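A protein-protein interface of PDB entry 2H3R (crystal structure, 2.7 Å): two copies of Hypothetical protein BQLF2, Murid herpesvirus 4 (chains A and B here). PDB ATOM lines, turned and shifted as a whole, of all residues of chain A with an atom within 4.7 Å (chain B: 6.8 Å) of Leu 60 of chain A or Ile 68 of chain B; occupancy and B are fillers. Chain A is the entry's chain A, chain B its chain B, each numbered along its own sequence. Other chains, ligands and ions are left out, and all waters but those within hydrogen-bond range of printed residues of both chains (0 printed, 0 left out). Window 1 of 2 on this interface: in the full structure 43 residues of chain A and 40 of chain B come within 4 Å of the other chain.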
ATOM      1  N   SER A  56     -28.366  10.194  -9.285  1.00  0.00           N
ATOM      2  CA  SER A  56     -29.186  11.393  -9.154  1.00  0.00           C
ATOM      3  C   SER A  56     -28.447  12.474  -8.370  1.00  0.00           C
ATOM      4  O   SER A  56     -28.450  13.645  -8.750  1.00  0.00           O
ATOM      5  CB  SER A  56     -30.504  11.047  -8.453  1.00  0.00           C
ATOM      6  OG  SER A  56     -31.168  10.002  -9.124  1.00  0.00           O
ATOM      7  N   SER A  57     -27.821  12.071  -7.268  1.00  0.00           N
ATOM      8  CA  SER A  57     -27.089  13.008  -6.437  1.00  0.00           C
ATOM      9  C   SER A  57     -26.013  13.669  -7.271  1.00  0.00           C
ATOM     10  O   SER A  57     -25.902  14.893  -7.299  1.00  0.00           O
ATOM     11  CB  SER A  57     -26.444  12.283  -5.261  1.00  0.00           C
ATOM     12  OG  SER A  57     -27.425  11.658  -4.463  1.00  0.00           O
ATOM     13  N   ARG A  58     -25.224  12.855  -7.959  1.00  0.00           N
ATOM     14  CA  ARG A  58     -24.150  13.389  -8.778  1.00  0.00           C
ATOM     15  C   ARG A  58     -24.652  14.323  -9.871  1.00  0.00           C
ATOM     16  O   ARG A  58     -24.062  15.382 -10.106  1.00  0.00           O
ATOM     17  CB  ARG A  58     -23.313  12.255  -9.363  1.00  0.00           C
ATOM     18  CG  ARG A  58     -22.462  11.546  -8.314  1.00  0.00           C
ATOM     19  CD  ARG A  58     -21.531  10.502  -8.926  1.00  0.00           C
ATOM     20  NE  ARG A  58     -20.645   9.920  -7.921  1.00  0.00           N
ATOM     21  CZ  ARG A  58     -20.137   8.695  -7.986  1.00  0.00           C
ATOM     22  NH1 ARG A  58     -20.421   7.907  -9.011  1.00  0.00           N
ATOM     23  NH2 ARG A  58     -19.350   8.251  -7.025  1.00  0.00           N
ATOM     24  N   ALA A  59     -25.742  13.948 -10.535  1.00  0.00           N
ATOM     25  CA  ALA A  59     -26.306  14.801 -11.574  1.00  0.00           C
ATOM     26  C   ALA A  59     -26.704  16.130 -10.943  1.00  0.00           C
ATOM     27  O   ALA A  59     -26.300  17.193 -11.411  1.00  0.00           O
ATOM     28  CB  ALA A  59     -27.509  14.150 -12.200  1.00  0.00           C
ATOM     29  N   LEU A  60     -27.503  16.070  -9.883  1.00  0.00           N
ATOM     30  CA  LEU A  60     -27.920  17.294  -9.197  1.00  0.00           C
ATOM     31  C   LEU A  60     -26.696  18.033  -8.635  1.00  0.00           C
ATOM     32  O   LEU A  60     -26.705  19.253  -8.481  1.00  0.00           O
ATOM     33  CB  LEU A  60     -28.934  16.963  -8.096  1.00  0.00           C
ATOM     34  CG  LEU A  60     -30.296  16.583  -8.696  1.00  0.00           C
ATOM     35  CD1 LEU A  60     -31.266  16.040  -7.650  1.00  0.00           C
ATOM     36  CD2 LEU A  60     -30.867  17.819  -9.361  1.00  0.00           C
ATOM     37  N   GLY A  61     -25.633  17.283  -8.355  1.00  0.00           N
ATOM     38  CA  GLY A  61     -24.419  17.893  -7.849  1.00  0.00           C
ATOM     39  C   GLY A  61     -23.798  18.767  -8.915  1.00  0.00           C
ATOM     40  O   GLY A  61     -23.300  19.847  -8.629  1.00  0.00           O
ATOM     41  N   ALA A  62     -23.818  18.281 -10.152  1.00  0.00           N
ATOM     42  CA  ALA A  62     -23.267  19.008 -11.298  1.00  0.00           C
ATOM     43  C   ALA A  62     -24.007  20.324 -11.480  1.00  0.00           C
ATOM     44  O   ALA A  62     -23.391  21.367 -11.709  1.00  0.00           O
ATOM     45  CB  ALA A  62     -23.399  18.157 -12.568  1.00  0.00           C
ATOM     46  N   VAL A  63     -25.334  20.268 -11.398  1.00  0.00           N
ATOM     47  CA  VAL A  63     -26.145  21.469 -11.539  1.00  0.00           C
ATOM     48  C   VAL A  63     -25.742  22.413 -10.418  1.00  0.00           C
ATOM     49  O   VAL A  63     -25.528  23.605 -10.642  1.00  0.00           O
ATOM     50  CB  VAL A  63     -27.660  21.155 -11.434  1.00  0.00           C
ATOM     51  CG1 VAL A  63     -28.467  22.431 -11.587  1.00  0.00           C
ATOM     52  CG2 VAL A  63     -28.078  20.158 -12.524  1.00  0.00           C
ATOM     53  N   ALA A  64     -25.607  21.875  -9.211  1.00  0.00           N
ATOM     54  CA  ALA A  64     -25.197  22.687  -8.077  1.00  0.00           C
ATOM     55  C   ALA A  64     -23.820  23.299  -8.338  1.00  0.00           C
ATOM     56  O   ALA A  64     -23.598  24.493  -8.088  1.00  0.00           O
ATOM     57  CB  ALA A  64     -25.180  21.850  -6.815  1.00  0.00           C
ATOM     58  N   VAL A  98     -31.965  23.181  -6.972  1.00  0.00           N
ATOM     59  CA  VAL A  98     -31.562  22.205  -7.978  1.00  0.00           C
ATOM     60  C   VAL A  98     -32.751  21.302  -8.314  1.00  0.00           C
ATOM     61  O   VAL A  98     -33.515  20.908  -7.432  1.00  0.00           O
ATOM     62  CB  VAL A  98     -30.342  21.337  -7.505  1.00  0.00           C
ATOM     63  CG1 VAL A  98     -29.111  22.212  -7.359  1.00  0.00           C
ATOM     64  CG2 VAL A  98     -30.647  20.643  -6.192  1.00  0.00           C
ATOM     65  N   SER A  99     -32.905  20.989  -9.595  1.00  0.00           N
ATOM     66  CA  SER A  99     -34.008  20.160 -10.042  1.00  0.00           C
ATOM     67  C   SER A  99     -33.600  19.114 -11.050  1.00  0.00           C
ATOM     68  O   SER A  99     -32.726  19.357 -11.870  1.00  0.00           O
ATOM     69  CB  SER A  99     -35.093  21.034 -10.670  1.00  0.00           C
ATOM     70  OG  SER A  99     -36.126  20.242 -11.233  1.00  0.00           O
ATOM     71  N   MET A 100     -34.250  17.954 -10.985  1.00  0.00           N
ATOM     72  CA  MET A 100     -33.994  16.873 -11.930  1.00  0.00           C
ATOM     73  C   MET A 100     -34.408  17.359 -13.320  1.00  0.00           C
ATOM     74  O   MET A 100     -33.892  16.898 -14.332  1.00  0.00           O
ATOM     75  CB  MET A 100     -34.817  15.632 -11.582  1.00  0.00           C
ATOM     76  CG  MET A 100     -34.239  14.759 -10.497  1.00  0.00           C
ATOM     77  SD  MET A 100     -32.606  13.848 -11.034  1.00  0.00           S
ATOM     78  CE  MET A 100     -33.385  12.483 -12.175  1.00  0.00           C
ATOM     79  N   GLY B  61     -18.905  23.495  -3.939  1.00  0.00           N
ATOM     80  CA  GLY B  61     -19.619  22.489  -4.693  1.00  0.00           C
ATOM     81  C   GLY B  61     -19.629  21.197  -3.903  1.00  0.00           C
ATOM     82  O   GLY B  61     -20.684  20.621  -3.631  1.00  0.00           O
ATOM     83  N   VAL B  63     -19.524  20.697  -0.972  1.00  0.00           N
ATOM     84  CA  VAL B  63     -20.422  20.741   0.180  1.00  0.00           C
ATOM     85  C   VAL B  63     -21.880  20.591  -0.269  1.00  0.00           C
ATOM     86  O   VAL B  63     -22.658  19.843   0.333  1.00  0.00           O
ATOM     87  CB  VAL B  63     -20.285  22.058   0.996  1.00  0.00           C
ATOM     88  CG1 VAL B  63     -21.557  22.301   1.822  1.00  0.00           C
ATOM     89  CG2 VAL B  63     -19.088  21.973   1.925  1.00  0.00           C
ATOM     90  N   ALA B  64     -22.246  21.311  -1.322  1.00  0.00           N
ATOM     91  CA  ALA B  64     -23.606  21.244  -1.845  1.00  0.00           C
ATOM     92  C   ALA B  64     -23.872  19.808  -2.257  1.00  0.00           C
ATOM     93  O   ALA B  64     -24.973  19.283  -2.101  1.00  0.00           O
ATOM     94  CB  ALA B  64     -23.743  22.167  -3.047  1.00  0.00           C
ATOM     95  N   MET B  65     -22.830  19.171  -2.764  1.00  0.00           N
ATOM     96  CA  MET B  65     -22.915  17.805  -3.236  1.00  0.00           C
ATOM     97  C   MET B  65     -23.187  16.829  -2.098  1.00  0.00           C
ATOM     98  O   MET B  65     -23.900  15.837  -2.263  1.00  0.00           O
ATOM     99  CB  MET B  65     -21.603  17.454  -3.937  1.00  0.00           C
ATOM    100  CG  MET B  65     -21.778  16.944  -5.337  1.00  0.00           C
ATOM    101  SD  MET B  65     -22.554  15.202  -5.312  1.00  0.00           S
ATOM    102  CE  MET B  65     -21.274  14.299  -6.436  1.00  0.00           C
ATOM    103  N   ARG B  66     -22.631  17.142  -0.941  1.00  0.00           N
ATOM    104  CA  ARG B  66     -22.750  16.305   0.244  1.00  0.00           C
ATOM    105  C   ARG B  66     -24.146  16.306   0.850  1.00  0.00           C
ATOM    106  O   ARG B  66     -24.628  15.267   1.286  1.00  0.00           O
ATOM    107  CB  ARG B  66     -21.711  16.766   1.273  1.00  0.00           C
ATOM    108  CG  ARG B  66     -21.213  15.705   2.232  1.00  0.00           C
ATOM    109  CD  ARG B  66     -20.137  16.300   3.127  1.00  0.00           C
ATOM    110  NE  ARG B  66     -20.573  17.570   3.712  1.00  0.00           N
ATOM    111  CZ  ARG B  66     -19.770  18.440   4.322  1.00  0.00           C
ATOM    112  NH1 ARG B  66     -18.468  18.188   4.435  1.00  0.00           N
ATOM    113  NH2 ARG B  66     -20.273  19.571   4.812  1.00  0.00           N
ATOM    114  N   LYS B  67     -24.802  17.461   0.894  1.00  0.00           N
ATOM    115  CA  LYS B  67     -26.148  17.502   1.465  1.00  0.00           C
ATOM    116  C   LYS B  67     -27.232  17.137   0.456  1.00  0.00           C
ATOM    117  O   LYS B  67     -28.331  16.738   0.837  1.00  0.00           O
ATOM    118  CB  LYS B  67     -26.444  18.860   2.108  1.00  0.00           C
ATOM    119  CG  LYS B  67     -26.154  20.068   1.269  1.00  0.00           C
ATOM    120  CD  LYS B  67     -26.876  21.282   1.861  1.00  0.00           C
ATOM    121  CE  LYS B  67     -26.375  21.682   3.238  1.00  0.00           C
ATOM    122  NZ  LYS B  67     -25.230  22.632   3.166  1.00  0.00           N
ATOM    123  N   ILE B  68     -26.927  17.271  -0.829  1.00  0.00           N
ATOM    124  CA  ILE B  68     -27.880  16.883  -1.850  1.00  0.00           C
ATOM    125  C   ILE B  68     -28.059  15.370  -1.724  1.00  0.00           C
ATOM    126  O   ILE B  68     -29.183  14.876  -1.671  1.00  0.00           O
ATOM    127  CB  ILE B  68     -27.374  17.220  -3.276  1.00  0.00           C
ATOM    128  CG1 ILE B  68     -27.500  18.716  -3.541  1.00  0.00           C
ATOM    129  CG2 ILE B  68     -28.189  16.451  -4.329  1.00  0.00           C
ATOM    130  CD1 ILE B  68     -26.693  19.230  -4.732  1.00  0.00           C
ATOM    131  N   GLU B  69     -26.953  14.630  -1.671  1.00  0.00           N
ATOM    132  CA  GLU B  69     -27.064  13.182  -1.538  1.00  0.00           C
ATOM    133  C   GLU B  69     -27.878  12.851  -0.302  1.00  0.00           C
ATOM    134  O   GLU B  69     -28.550  11.826  -0.242  1.00  0.00           O
ATOM    135  CB  GLU B  69     -25.687  12.506  -1.430  1.00  0.00           C
ATOM    136  CG  GLU B  69     -25.824  10.998  -1.196  1.00  0.00           C
ATOM    137  CD  GLU B  69     -24.496  10.249  -1.169  1.00  0.00           C
ATOM    138  OE1 GLU B  69     -24.484   9.084  -0.703  1.00  0.00           O
ATOM    139  OE2 GLU B  69     -23.471  10.810  -1.618  1.00  0.00           O
ATOM    140  N   ALA B  70     -27.817  13.727   0.692  1.00  0.00           N
ATOM    141  CA  ALA B  70     -28.550  13.510   1.932  1.00  0.00           C
ATOM    142  C   ALA B  70     -30.046  13.699   1.717  1.00  0.00           C
ATOM    143  O   ALA B  70     -30.848  12.915   2.218  1.00  0.00           O
ATOM    144  CB  ALA B  70     -28.047  14.467   3.025  1.00  0.00           C
ATOM    145  N   LYS B  71     -30.425  14.733   0.971  1.00  0.00           N
ATOM    146  CA  LYS B  71     -31.838  14.989   0.708  1.00  0.00           C
ATOM    147  C   LYS B  71     -32.456  13.964  -0.251  1.00  0.00           C
ATOM    148  O   LYS B  71     -33.610  13.568  -0.089  1.00  0.00           O
ATOM    149  CB  LYS B  71     -32.028  16.408   0.171  1.00  0.00           C
ATOM    150  CG  LYS B  71     -31.531  17.470   1.128  1.00  0.00           C
ATOM    151  CD  LYS B  71     -32.087  18.850   0.810  1.00  0.00           C
ATOM    152  CE  LYS B  71     -31.649  19.844   1.879  1.00  0.00           C
ATOM    153  NZ  LYS B  71     -32.393  21.131   1.836  1.00  0.00           N
ATOM    154  N   VAL B  72     -31.686  13.536  -1.244  1.00  0.00           N
ATOM    155  CA  VAL B  72     -32.177  12.554  -2.199  1.00  0.00           C
ATOM    156  C   VAL B  72     -32.381  11.223  -1.489  1.00  0.00           C
ATOM    157  O   VAL B  72     -33.458  10.638  -1.553  1.00  0.00           O
ATOM    158  CB  VAL B  72     -31.177  12.351  -3.366  1.00  0.00           C
ATOM    159  CG1 VAL B  72     -31.451  11.040  -4.072  1.00  0.00           C
ATOM    160  CG2 VAL B  72     -31.281  13.499  -4.347  1.00  0.00           C
ATOM    161  N   ARG B  73     -31.348  10.752  -0.793  1.00  0.00           N
ATOM    162  CA  ARG B  73     -31.443   9.469  -0.104  1.00  0.00           C
ATOM    163  C   ARG B  73     -32.627   9.454   0.859  1.00  0.00           C
ATOM    164  O   ARG B  73     -33.376   8.485   0.926  1.00  0.00           O
ATOM    165  CB  ARG B  73     -30.139   9.139   0.650  1.00  0.00           C
ATOM    166  CG  ARG B  73     -30.131   7.697   1.147  1.00  0.00           C
ATOM    167  CD  ARG B  73     -28.862   7.279   1.858  1.00  0.00           C
ATOM    168  NE  ARG B  73     -27.840   6.698   0.989  1.00  0.00           N
ATOM    169  CZ  ARG B  73     -26.811   7.384   0.500  1.00  0.00           C
ATOM    170  NH1 ARG B  73     -26.678   8.676   0.787  1.00  0.00           N
ATOM    171  NH2 ARG B  73     -25.890   6.775  -0.238  1.00  0.00           N
ATOM    172  N   SER B  74     -32.787  10.543   1.604  1.00  0.00           N
ATOM    173  CA  SER B  74     -33.887  10.668   2.552  1.00  0.00           C
ATOM    174  C   SER B  74     -35.233  10.691   1.836  1.00  0.00           C
ATOM    175  O   SER B  74     -36.217  10.136   2.325  1.00  0.00           O
ATOM    176  CB  SER B  74     -33.721  11.929   3.402  1.00  0.00           C
ATOM    177  OG  SER B  74     -34.978  12.421   3.835  1.00  0.00           O
ATOM    178  N   LEU B  89     -38.495  10.941  -9.062  1.00  0.00           N
ATOM    179  CA  LEU B  89     -37.288  11.604  -9.556  1.00  0.00           C
ATOM    180  C   LEU B  89     -37.476  12.378 -10.844  1.00  0.00           C
ATOM    181  O   LEU B  89     -36.537  12.993 -11.345  1.00  0.00           O
ATOM    182  CB  LEU B  89     -36.173  10.578  -9.744  1.00  0.00           C
ATOM    183  CG  LEU B  89     -35.531  10.149  -8.434  1.00  0.00           C
ATOM    184  CD1 LEU B  89     -34.738   8.876  -8.612  1.00  0.00           C
ATOM    185  CD2 LEU B  89     -34.662  11.290  -7.946  1.00  0.00           C
ATOM    186  N   LEU B  92     -38.015  16.034  -9.043  1.00  0.00           N
ATOM    187  CA  LEU B  92     -37.568  16.305  -7.684  1.00  0.00           C
ATOM    188  C   LEU B  92     -36.763  17.597  -7.620  1.00  0.00           C
ATOM    189  O   LEU B  92     -35.899  17.833  -8.465  1.00  0.00           O
ATOM    190  CB  LEU B  92     -36.679  15.175  -7.188  1.00  0.00           C
ATOM    191  CG  LEU B  92     -35.916  15.529  -5.916  1.00  0.00           C
ATOM    192  CD1 LEU B  92     -36.826  15.329  -4.722  1.00  0.00           C
ATOM    193  CD2 LEU B  92     -34.673  14.664  -5.795  1.00  0.00           C
ATOM    194  N   THR B  93     -37.033  18.421  -6.608  1.00  0.00           N
ATOM    195  CA  THR B  93     -36.307  19.678  -6.443  1.00  0.00           C
ATOM    196  C   THR B  93     -35.773  19.835  -5.025  1.00  0.00           C
ATOM    197  O   THR B  93     -36.400  19.395  -4.063  1.00  0.00           O
ATOM    198  CB  THR B  93     -37.190  20.886  -6.744  1.00  0.00           C
ATOM    199  OG1 THR B  93     -37.822  20.706  -8.011  1.00  0.00           O
ATOM    200  CG2 THR B  93     -36.357  22.143  -6.799  1.00  0.00           C
ATOM    201  N   LEU B  94     -34.624  20.479  -4.886  1.00  0.00           N
ATOM    202  CA  LEU B  94     -34.044  20.666  -3.576  1.00  0.00           C
ATOM    203  C   LEU B  94     -33.512  22.074  -3.392  1.00  0.00           C
ATOM    204  O   LEU B  94     -32.973  22.676  -4.321  1.00  0.00           O
ATOM    205  CB  LEU B  94     -32.900  19.673  -3.373  1.00  0.00           C
ATOM    206  CG  LEU B  94     -33.147  18.186  -3.625  1.00  0.00           C
ATOM    207  CD1 LEU B  94     -31.800  17.473  -3.781  1.00  0.00           C
ATOM    208  CD2 LEU B  94     -33.969  17.584  -2.500  1.00  0.00           C
ATOM    209  N   VAL B  96     -30.777  24.211  -1.485  1.00  0.00           N
ATOM    210  CA  VAL B  96     -29.520  23.912  -0.808  1.00  0.00           C
ATOM    211  C   VAL B  96     -28.706  25.148  -0.525  1.00  0.00           C
ATOM    212  O   VAL B  96     -28.506  26.005  -1.382  1.00  0.00           O
ATOM    213  CB  VAL B  96     -28.653  22.917  -1.610  1.00  0.00           C
ATOM    214  CG1 VAL B  96     -27.414  23.621  -2.158  1.00  0.00           C
ATOM    215  CG2 VAL B  96     -28.268  21.740  -0.729  1.00  0.00           C
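The backbone carbonyl oxygen (O) of Val 98 of chain A sits at hydrogen-bond distance from the backbone NH (N) of Leu 94 of chain B, at 2.8 Å. The backbone NH (N) of Met 100 of chain A is in hydrogen-bond range of the backbone carbonyl oxygen (O) of Leu 92 of chain B.
Printed residues of chain B within 4 Å of Ser 56 of chain A: Leu 89. Of the printed residues of chain B, Arg 58 of chain A touches Met 65 (3.5 Å). Leu 60 of chain A touches one residue of chain B. Of the printed residues of chain B, Ala 64 of chain A touches Ile 68. Ile 68 of chain B touches two residues of chain A. Printed residues of chain A within 4 Å of Leu 89 of chain B: Ser 56 (3.8 Å) and Met 100 (3.0 Å). The nearest printed residue of chain A that does not touch Ile 68 of chain B is Ser 57 of chain A (4.1 Å). The nearest printed residue of chain A that does not touch Glu 69 of chain B is Arg 58 of chain A (6.6 Å).
Of the 12 printed residues of chain A, 9 touch a printed residue of chain B. Printed residues of chain A that touch a printed residue of chain B: Ser 56, Ser 57, Arg 58, Leu 60, Gly 61, Ala 64, Val 98, Ser 99 and Met 100. Hydrophobic or aromatic side chains of chain A that line the printed part of chain B: Leu 60, Ala 64, Val 98 and Met 100. Among the printed residues, 14 pairs touch across the chains. Among the printed residues, no Asp or Glu carboxylate lies within 4 Å of a Lys or Arg side-chain nitrogen of the other chain.
NH1 of Arg 73 of chain B is in salt-bridge range of OE1 of Glu 69 of chain B (2.7 Å).
Positions printed for both chains: 61, 63 and 64. Of the 14 pairs that touch across the chains among the printed residues, none has its exchanged pair printed and touching as well.
OG of Ser 56 of chain A touches CD1 of Leu 89 of chain B (3.8 Å). Ser 57 of chain A touches Met 65 of chain B (O to SD, 3.9 Å). OG of Ser 57 of chain A touches CA of Glu 69 of chain B (3.3 Å). CB of Val 72 of chain B touches OG of Ser 57 of chain A, 3.97 Å away. Leu 60 of chain A touches Ile 68 of chain B. Met 65 of chain B touches Gly 61 of chain A. Ala 64 of chain A touches Ile 68 of chain B (CB to CD1, 3.7 Å). O of Val 98 of chain A touches CG2 of Thr 93 of chain B, at 3.2 Å. Leu 92 of chain B touches Ser 99 of chain A (O to CA, 3.4 Å). Met 100 of chain A touches Leu 89 of chain B.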
